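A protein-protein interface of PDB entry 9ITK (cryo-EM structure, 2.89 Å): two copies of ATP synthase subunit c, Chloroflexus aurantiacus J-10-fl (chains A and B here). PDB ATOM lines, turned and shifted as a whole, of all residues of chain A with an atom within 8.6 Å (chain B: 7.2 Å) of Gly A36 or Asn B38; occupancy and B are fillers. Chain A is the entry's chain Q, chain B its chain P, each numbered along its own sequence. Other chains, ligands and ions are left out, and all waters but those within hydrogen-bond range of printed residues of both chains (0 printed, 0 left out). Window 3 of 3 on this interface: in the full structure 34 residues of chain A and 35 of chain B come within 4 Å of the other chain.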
ATOM      1  N   SER A  29      -3.052   4.277  30.632  1.00  0.00           N
ATOM      2  CA  SER A  29      -1.631   4.319  30.305  1.00  0.00           C
ATOM      3  C   SER A  29      -1.275   3.277  29.257  1.00  0.00           C
ATOM      4  O   SER A  29      -0.498   3.552  28.336  1.00  0.00           O
ATOM      5  CB  SER A  29      -0.793   4.111  31.562  1.00  0.00           C
ATOM      6  OG  SER A  29       0.587   4.087  31.249  1.00  0.00           O
ATOM      7  N   GLY A  30      -1.826   2.070  29.382  1.00  0.00           N
ATOM      8  CA  GLY A  30      -1.608   1.067  28.355  1.00  0.00           C
ATOM      9  C   GLY A  30      -2.213   1.464  27.022  1.00  0.00           C
ATOM     10  O   GLY A  30      -1.656   1.168  25.964  1.00  0.00           O
ATOM     11  N   ALA A  31      -3.365   2.135  27.055  1.00  0.00           N
ATOM     12  CA  ALA A  31      -4.015   2.556  25.819  1.00  0.00           C
ATOM     13  C   ALA A  31      -3.260   3.698  25.152  1.00  0.00           C
ATOM     14  O   ALA A  31      -2.997   3.657  23.945  1.00  0.00           O
ATOM     15  CB  ALA A  31      -5.460   2.958  26.095  1.00  0.00           C
ATOM     16  N   VAL A  32      -2.896   4.726  25.923  1.00  0.00           N
ATOM     17  CA  VAL A  32      -2.261   5.898  25.328  1.00  0.00           C
ATOM     18  C   VAL A  32      -0.896   5.547  24.752  1.00  0.00           C
ATOM     19  O   VAL A  32      -0.440   6.177  23.791  1.00  0.00           O
ATOM     20  CB  VAL A  32      -2.164   7.047  26.348  1.00  0.00           C
ATOM     21  CG1 VAL A  32      -3.548   7.434  26.834  1.00  0.00           C
ATOM     22  CG2 VAL A  32      -1.268   6.670  27.509  1.00  0.00           C
ATOM     23  N   GLN A  33      -0.214   4.554  25.327  1.00  0.00           N
ATOM     24  CA  GLN A  33       1.014   4.065  24.714  1.00  0.00           C
ATOM     25  C   GLN A  33       0.731   3.455  23.349  1.00  0.00           C
ATOM     26  O   GLN A  33       1.484   3.677  22.393  1.00  0.00           O
ATOM     27  CB  GLN A  33       1.688   3.042  25.628  1.00  0.00           C
ATOM     28  CG  GLN A  33       2.317   3.618  26.886  1.00  0.00           C
ATOM     29  CD  GLN A  33       3.584   4.395  26.606  1.00  0.00           C
ATOM     30  OE1 GLN A  33       4.607   3.821  26.234  1.00  0.00           O
ATOM     31  NE2 GLN A  33       3.528   5.708  26.794  1.00  0.00           N
ATOM     32  N   ALA A  34      -0.354   2.686  23.235  1.00  0.00           N
ATOM     33  CA  ALA A  34      -0.702   2.075  21.957  1.00  0.00           C
ATOM     34  C   ALA A  34      -1.180   3.109  20.948  1.00  0.00           C
ATOM     35  O   ALA A  34      -0.978   2.933  19.741  1.00  0.00           O
ATOM     36  CB  ALA A  34      -1.766   0.999  22.160  1.00  0.00           C
ATOM     37  N   ILE A  35      -1.824   4.182  21.414  1.00  0.00           N
ATOM     38  CA  ILE A  35      -2.238   5.251  20.510  1.00  0.00           C
ATOM     39  C   ILE A  35      -1.022   5.902  19.867  1.00  0.00           C
ATOM     40  O   ILE A  35      -1.014   6.186  18.663  1.00  0.00           O
ATOM     41  CB  ILE A  35      -3.103   6.283  21.258  1.00  0.00           C
ATOM     42  CG1 ILE A  35      -4.385   5.634  21.782  1.00  0.00           C
ATOM     43  CG2 ILE A  35      -3.426   7.463  20.361  1.00  0.00           C
ATOM     44  CD1 ILE A  35      -5.083   4.760  20.772  1.00  0.00           C
ATOM     45  N   GLY A  36       0.024   6.149  20.657  1.00  0.00           N
ATOM     46  CA  GLY A  36       1.229   6.747  20.108  1.00  0.00           C
ATOM     47  C   GLY A  36       1.889   5.877  19.057  1.00  0.00           C
ATOM     48  O   GLY A  36       2.363   6.374  18.034  1.00  0.00           O
ATOM     49  N   ARG A  37       1.931   4.566  19.294  1.00  0.00           N
ATOM     50  CA  ARG A  37       2.547   3.662  18.329  1.00  0.00           C
ATOM     51  C   ARG A  37       1.746   3.607  17.033  1.00  0.00           C
ATOM     52  O   ARG A  37       2.318   3.629  15.938  1.00  0.00           O
ATOM     53  CB  ARG A  37       2.690   2.268  18.936  1.00  0.00           C
ATOM     54  CG  ARG A  37       3.467   2.240  20.242  1.00  0.00           C
ATOM     55  CD  ARG A  37       4.231   0.934  20.431  1.00  0.00           C
ATOM     56  NE  ARG A  37       5.042   0.579  19.271  1.00  0.00           N
ATOM     57  CZ  ARG A  37       4.688  -0.298  18.343  1.00  0.00           C
ATOM     58  NH1 ARG A  37       3.531  -0.938  18.402  1.00  0.00           N
ATOM     59  NH2 ARG A  37       5.514  -0.540  17.329  1.00  0.00           N
ATOM     60  N   ASN A  38       0.420   3.540  17.137  1.00  0.00           N
ATOM     61  CA  ASN A  38      -0.449   3.408  15.968  1.00  0.00           C
ATOM     62  C   ASN A  38      -1.722   4.212  16.178  1.00  0.00           C
ATOM     63  O   ASN A  38      -2.718   3.702  16.708  1.00  0.00           O
ATOM     64  CB  ASN A  38      -0.782   1.941  15.691  1.00  0.00           C
ATOM     65  CG  ASN A  38       0.322   1.226  14.950  1.00  0.00           C
ATOM     66  OD1 ASN A  38       1.041   1.827  14.154  1.00  0.00           O
ATOM     67  ND2 ASN A  38       0.463  -0.067  15.206  1.00  0.00           N
ATOM     68  N   PRO A  39      -1.730   5.483  15.768  1.00  0.00           N
ATOM     69  CA  PRO A  39      -2.964   6.277  15.874  1.00  0.00           C
ATOM     70  C   PRO A  39      -4.094   5.758  15.006  1.00  0.00           C
ATOM     71  O   PRO A  39      -5.253   6.117  15.246  1.00  0.00           O
ATOM     72  CB  PRO A  39      -2.523   7.680  15.432  1.00  0.00           C
ATOM     73  CG  PRO A  39      -1.030   7.682  15.574  1.00  0.00           C
ATOM     74  CD  PRO A  39      -0.600   6.282  15.269  1.00  0.00           C
ATOM     75  N   GLU A  40      -3.794   4.930  14.002  1.00  0.00           N
ATOM     76  CA  GLU A  40      -4.825   4.458  13.083  1.00  0.00           C
ATOM     77  C   GLU A  40      -5.831   3.549  13.779  1.00  0.00           C
ATOM     78  O   GLU A  40      -7.023   3.567  13.450  1.00  0.00           O
ATOM     79  CB  GLU A  40      -4.172   3.734  11.906  1.00  0.00           C
ATOM     80  CG  GLU A  40      -5.140   3.289  10.825  1.00  0.00           C
ATOM     81  CD  GLU A  40      -4.437   2.629   9.655  1.00  0.00           C
ATOM     82  OE1 GLU A  40      -3.202   2.461   9.722  1.00  0.00           O
ATOM     83  OE2 GLU A  40      -5.119   2.281   8.667  1.00  0.00           O
ATOM     84  N   GLU A  42      -6.821   3.626  16.722  1.00  0.00           N
ATOM     85  CA  GLU A  42      -7.397   4.285  17.890  1.00  0.00           C
ATOM     86  C   GLU A  42      -8.881   3.977  18.036  1.00  0.00           C
ATOM     87  O   GLU A  42      -9.360   3.701  19.143  1.00  0.00           O
ATOM     88  CB  GLU A  42      -7.199   5.795  17.790  1.00  0.00           C
ATOM     89  CG  GLU A  42      -8.048   6.578  18.772  1.00  0.00           C
ATOM     90  CD  GLU A  42      -7.982   8.064  18.535  1.00  0.00           C
ATOM     91  OE1 GLU A  42      -7.277   8.480  17.595  1.00  0.00           O
ATOM     92  OE2 GLU A  42      -8.638   8.819  19.282  1.00  0.00           O
ATOM     93  N   VAL A  45      -9.742   0.513  19.918  1.00  0.00           N
ATOM     94  CA  VAL A  45      -9.115   0.231  21.206  1.00  0.00           C
ATOM     95  C   VAL A  45      -9.680   1.134  22.296  1.00  0.00           C
ATOM     96  O   VAL A  45      -9.795   0.714  23.452  1.00  0.00           O
ATOM     97  CB  VAL A  45      -7.584   0.357  21.119  1.00  0.00           C
ATOM     98  CG1 VAL A  45      -7.024  -0.650  20.135  1.00  0.00           C
ATOM     99  CG2 VAL A  45      -7.173   1.769  20.739  1.00  0.00           C
ATOM    100  N   GLN B  33       5.147   9.868  28.091  1.00  0.00           N
ATOM    101  CA  GLN B  33       6.028   9.120  27.204  1.00  0.00           C
ATOM    102  C   GLN B  33       5.419   8.977  25.816  1.00  0.00           C
ATOM    103  O   GLN B  33       6.145   8.963  24.815  1.00  0.00           O
ATOM    104  CB  GLN B  33       6.330   7.748  27.805  1.00  0.00           C
ATOM    105  CG  GLN B  33       7.316   7.788  28.955  1.00  0.00           C
ATOM    106  CD  GLN B  33       7.520   6.431  29.590  1.00  0.00           C
ATOM    107  OE1 GLN B  33       6.798   5.482  29.294  1.00  0.00           O
ATOM    108  NE2 GLN B  33       8.507   6.333  30.469  1.00  0.00           N
ATOM    109  N   ALA B  34       4.092   8.869  25.735  1.00  0.00           N
ATOM    110  CA  ALA B  34       3.440   8.698  24.442  1.00  0.00           C
ATOM    111  C   ALA B  34       3.623   9.924  23.555  1.00  0.00           C
ATOM    112  O   ALA B  34       3.927   9.792  22.364  1.00  0.00           O
ATOM    113  CB  ALA B  34       1.956   8.397  24.637  1.00  0.00           C
ATOM    114  N   ILE B  35       3.441  11.124  24.112  1.00  0.00           N
ATOM    115  CA  ILE B  35       3.608  12.330  23.309  1.00  0.00           C
ATOM    116  C   ILE B  35       5.071  12.539  22.944  1.00  0.00           C
ATOM    117  O   ILE B  35       5.377  13.144  21.910  1.00  0.00           O
ATOM    118  CB  ILE B  35       3.026  13.560  24.035  1.00  0.00           C
ATOM    119  CG1 ILE B  35       3.893  13.954  25.230  1.00  0.00           C
ATOM    120  CG2 ILE B  35       1.603  13.295  24.480  1.00  0.00           C
ATOM    121  CD1 ILE B  35       3.509  15.277  25.843  1.00  0.00           C
ATOM    122  N   GLY B  36       5.994  12.050  23.773  1.00  0.00           N
ATOM    123  CA  GLY B  36       7.405  12.188  23.451  1.00  0.00           C
ATOM    124  C   GLY B  36       7.784  11.455  22.179  1.00  0.00           C
ATOM    125  O   GLY B  36       8.569  11.955  21.371  1.00  0.00           O
ATOM    126  N   ARG B  37       7.234  10.256  21.986  1.00  0.00           N
ATOM    127  CA  ARG B  37       7.514   9.495  20.776  1.00  0.00           C
ATOM    128  C   ARG B  37       6.735  10.027  19.578  1.00  0.00           C
ATOM    129  O   ARG B  37       7.255  10.042  18.456  1.00  0.00           O
ATOM    130  CB  ARG B  37       7.203   8.017  21.006  1.00  0.00           C
ATOM    131  CG  ARG B  37       7.956   7.417  22.179  1.00  0.00           C
ATOM    132  CD  ARG B  37       8.245   5.944  21.957  1.00  0.00           C
ATOM    133  NE  ARG B  37       7.173   5.099  22.470  1.00  0.00           N
ATOM    134  CZ  ARG B  37       7.021   4.776  23.747  1.00  0.00           C
ATOM    135  NH1 ARG B  37       7.860   5.209  24.673  1.00  0.00           N
ATOM    136  NH2 ARG B  37       6.001   4.000  24.102  1.00  0.00           N
ATOM    137  N   ASN B  38       5.498  10.469  19.790  1.00  0.00           N
ATOM    138  CA  ASN B  38       4.635  10.972  18.720  1.00  0.00           C
ATOM    139  C   ASN B  38       4.096  12.339  19.118  1.00  0.00           C
ATOM    140  O   ASN B  38       2.971  12.456  19.621  1.00  0.00           O
ATOM    141  CB  ASN B  38       3.492  10.002  18.424  1.00  0.00           C
ATOM    142  CG  ASN B  38       3.906   8.888  17.492  1.00  0.00           C
ATOM    143  OD1 ASN B  38       5.089   8.579  17.361  1.00  0.00           O
ATOM    144  ND2 ASN B  38       2.929   8.277  16.831  1.00  0.00           N
ATOM    145  N   PRO B  39       4.875  13.400  18.903  1.00  0.00           N
ATOM    146  CA  PRO B  39       4.410  14.743  19.284  1.00  0.00           C
ATOM    147  C   PRO B  39       3.178  15.203  18.525  1.00  0.00           C
ATOM    148  O   PRO B  39       2.495  16.125  18.987  1.00  0.00           O
ATOM    149  CB  PRO B  39       5.621  15.637  18.978  1.00  0.00           C
ATOM    150  CG  PRO B  39       6.785  14.701  18.851  1.00  0.00           C
ATOM    151  CD  PRO B  39       6.226  13.425  18.321  1.00  0.00           C
ATOM    152  N   GLU B  40       2.869  14.592  17.379  1.00  0.00           N
ATOM    153  CA  GLU B  40       1.790  15.085  16.532  1.00  0.00           C
ATOM    154  C   GLU B  40       0.407  14.807  17.108  1.00  0.00           C
ATOM    155  O   GLU B  40      -0.549  15.497  16.740  1.00  0.00           O
ATOM    156  CB  GLU B  40       1.906  14.468  15.137  1.00  0.00           C
ATOM    157  CG  GLU B  40       1.281  13.088  15.013  1.00  0.00           C
ATOM    158  CD  GLU B  40       2.156  11.995  15.596  1.00  0.00           C
ATOM    159  OE1 GLU B  40       3.289  12.299  16.022  1.00  0.00           O
ATOM    160  OE2 GLU B  40       1.706  10.830  15.632  1.00  0.00           O
ATOM    161  N   ILE B  41       0.270  13.827  17.997  1.00  0.00           N
ATOM    162  CA  ILE B  41      -1.028  13.468  18.551  1.00  0.00           C
ATOM    163  C   ILE B  41      -1.173  13.959  19.990  1.00  0.00           C
ATOM    164  O   ILE B  41      -2.014  13.456  20.733  1.00  0.00           O
ATOM    165  CB  ILE B  41      -1.280  11.955  18.454  1.00  0.00           C
ATOM    166  CG1 ILE B  41      -0.240  11.191  19.269  1.00  0.00           C
ATOM    167  CG2 ILE B  41      -1.264  11.502  17.004  1.00  0.00           C
ATOM    168  CD1 ILE B  41      -0.557   9.729  19.412  1.00  0.00           C
ATOM    169  N   GLU B  42      -0.363  14.940  20.388  1.00  0.00           N
ATOM    170  CA  GLU B  42      -0.440  15.467  21.747  1.00  0.00           C
ATOM    171  C   GLU B  42      -1.807  16.073  22.030  1.00  0.00           C
ATOM    172  O   GLU B  42      -2.403  15.824  23.083  1.00  0.00           O
ATOM    173  CB  GLU B  42       0.670  16.496  21.961  1.00  0.00           C
ATOM    174  CG  GLU B  42       0.843  16.954  23.394  1.00  0.00           C
ATOM    175  CD  GLU B  42      -0.115  18.064  23.769  1.00  0.00           C
ATOM    176  OE1 GLU B  42      -0.512  18.834  22.870  1.00  0.00           O
ATOM    177  OE2 GLU B  42      -0.464  18.176  24.959  1.00  0.00           O
ATOM    178  N   ASN B  43      -2.330  16.863  21.093  1.00  0.00           N
ATOM    179  CA  ASN B  43      -3.633  17.486  21.294  1.00  0.00           C
ATOM    180  C   ASN B  43      -4.761  16.465  21.307  1.00  0.00           C
ATOM    181  O   ASN B  43      -5.891  16.810  21.670  1.00  0.00           O
ATOM    182  CB  ASN B  43      -3.882  18.536  20.212  1.00  0.00           C
ATOM    183  CG  ASN B  43      -2.759  19.552  20.118  1.00  0.00           C
ATOM    184  OD1 ASN B  43      -2.574  20.373  21.016  1.00  0.00           O
ATOM    185  ND2 ASN B  43      -1.998  19.494  19.032  1.00  0.00           N
ATOM    186  N   ARG B  44      -4.484  15.223  20.917  1.00  0.00           N
ATOM    187  CA  ARG B  44      -5.510  14.194  20.829  1.00  0.00           C
ATOM    188  C   ARG B  44      -5.438  13.176  21.958  1.00  0.00           C
ATOM    189  O   ARG B  44      -6.482  12.691  22.409  1.00  0.00           O
ATOM    190  CB  ARG B  44      -5.406  13.486  19.475  1.00  0.00           C
ATOM    191  CG  ARG B  44      -6.681  12.820  18.990  1.00  0.00           C
ATOM    192  CD  ARG B  44      -6.768  11.390  19.489  1.00  0.00           C
ATOM    193  NE  ARG B  44      -5.527  10.669  19.232  1.00  0.00           N
ATOM    194  CZ  ARG B  44      -5.095  10.315  18.030  1.00  0.00           C
ATOM    195  NH1 ARG B  44      -5.798  10.570  16.937  1.00  0.00           N
ATOM    196  NH2 ARG B  44      -3.931   9.681  17.919  1.00  0.00           N
ATOM    197  N   VAL B  45      -4.240  12.840  22.430  1.00  0.00           N
ATOM    198  CA  VAL B  45      -4.114  11.810  23.455  1.00  0.00           C
ATOM    199  C   VAL B  45      -4.245  12.393  24.862  1.00  0.00           C
ATOM    200  O   VAL B  45      -4.641  11.683  25.791  1.00  0.00           O
ATOM    201  CB  VAL B  45      -2.785  11.053  23.286  1.00  0.00           C
ATOM    202  CG1 VAL B  45      -1.604  11.972  23.534  1.00  0.00           C
ATOM    203  CG2 VAL B  45      -2.733   9.841  24.189  1.00  0.00           C
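NE2 of Gln A33 lies close to N of Ala B34 (3.4 Å).
NH2 of Arg B37 lies within hydrogen-bond range of OE1 of Gln A33, at 2.6 Å.
The guanidinium group (NH1) of Arg B44 lies within salt-bridge range of the side-chain carboxylate (OE1) of Glu A42 (2.6 Å).
The backbone carbonyl oxygen (O) of Gly A36 sits close to the side-chain amide nitrogen (ND2) of Asn B38 (2.3 Å).
The side-chain carboxylate (OE2) of Glu B40 sits at hydrogen-bond distance from the side-chain amide nitrogen (ND2) of Asn B38, at 3.1 Å.
Among the printed residues, merely in contact across the chains: Ile A35 with Arg B44, Val A32 with Ala B34, Pro A39 with Arg B44, Gly A36 with Ile B41, Val A32 with Val B45, Gln A33 with Gln B33 and Ile A35 with Ile B41.
Printed residues of chain B within 4 Å of Val A32: Ala B34 (3.4 Å) and Val B45 (3.6 Å).
Of the printed residues of chain B, Ile A35 touches Ile B41 and Arg B44.
Of chain B, only Asn B38 and Ile B41 come within 4 Å of Gly A36.
No residue of chain A comes within 4 Å of Gly B36.
Asn B38 touches one residue of chain A.
No residue of chain A comes within 4 Å of Pro B39.
Glu B40 touches none of the printed residues of chain A.
Of the printed residues of chain A, Ile B41 touches Ile A35 and Gly A36.
The nearest printed residue of chain B that does not touch Pro A39 is Ile B41 (4.1 Å).
Hydrophobic or aromatic side chains of chain B that line the printed part of chain A: Ala B34, Ile B41 and Val B45.
Among the printed residues, Asp or Glu carboxylates within 4 Å of a Lys or Arg side-chain nitrogen of the other chain: Glu A42 with Arg B44.
Gln A33 touches its own counterpart, Gln B33.
Gln A33 touches Ala B34, but with the chains exchanged Ala A34 does not touch Gln B33 (8.9 Å).
Gln A33 touches Arg B37, but with the chains exchanged Arg A37 does not touch Gln B33 (8.2 Å).
Gly A36 touches Asn B38, but with the chains exchanged Asn A38 does not touch Gly B36 (11.9 Å).
Positions printed for both chains: 33, 34, 35, 36, 37, 38, 39, 40, 42 and 45.
Of the 11 pairs that touch across the chains among the printed residues, 1 has its exchanged pair printed and touching as well.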
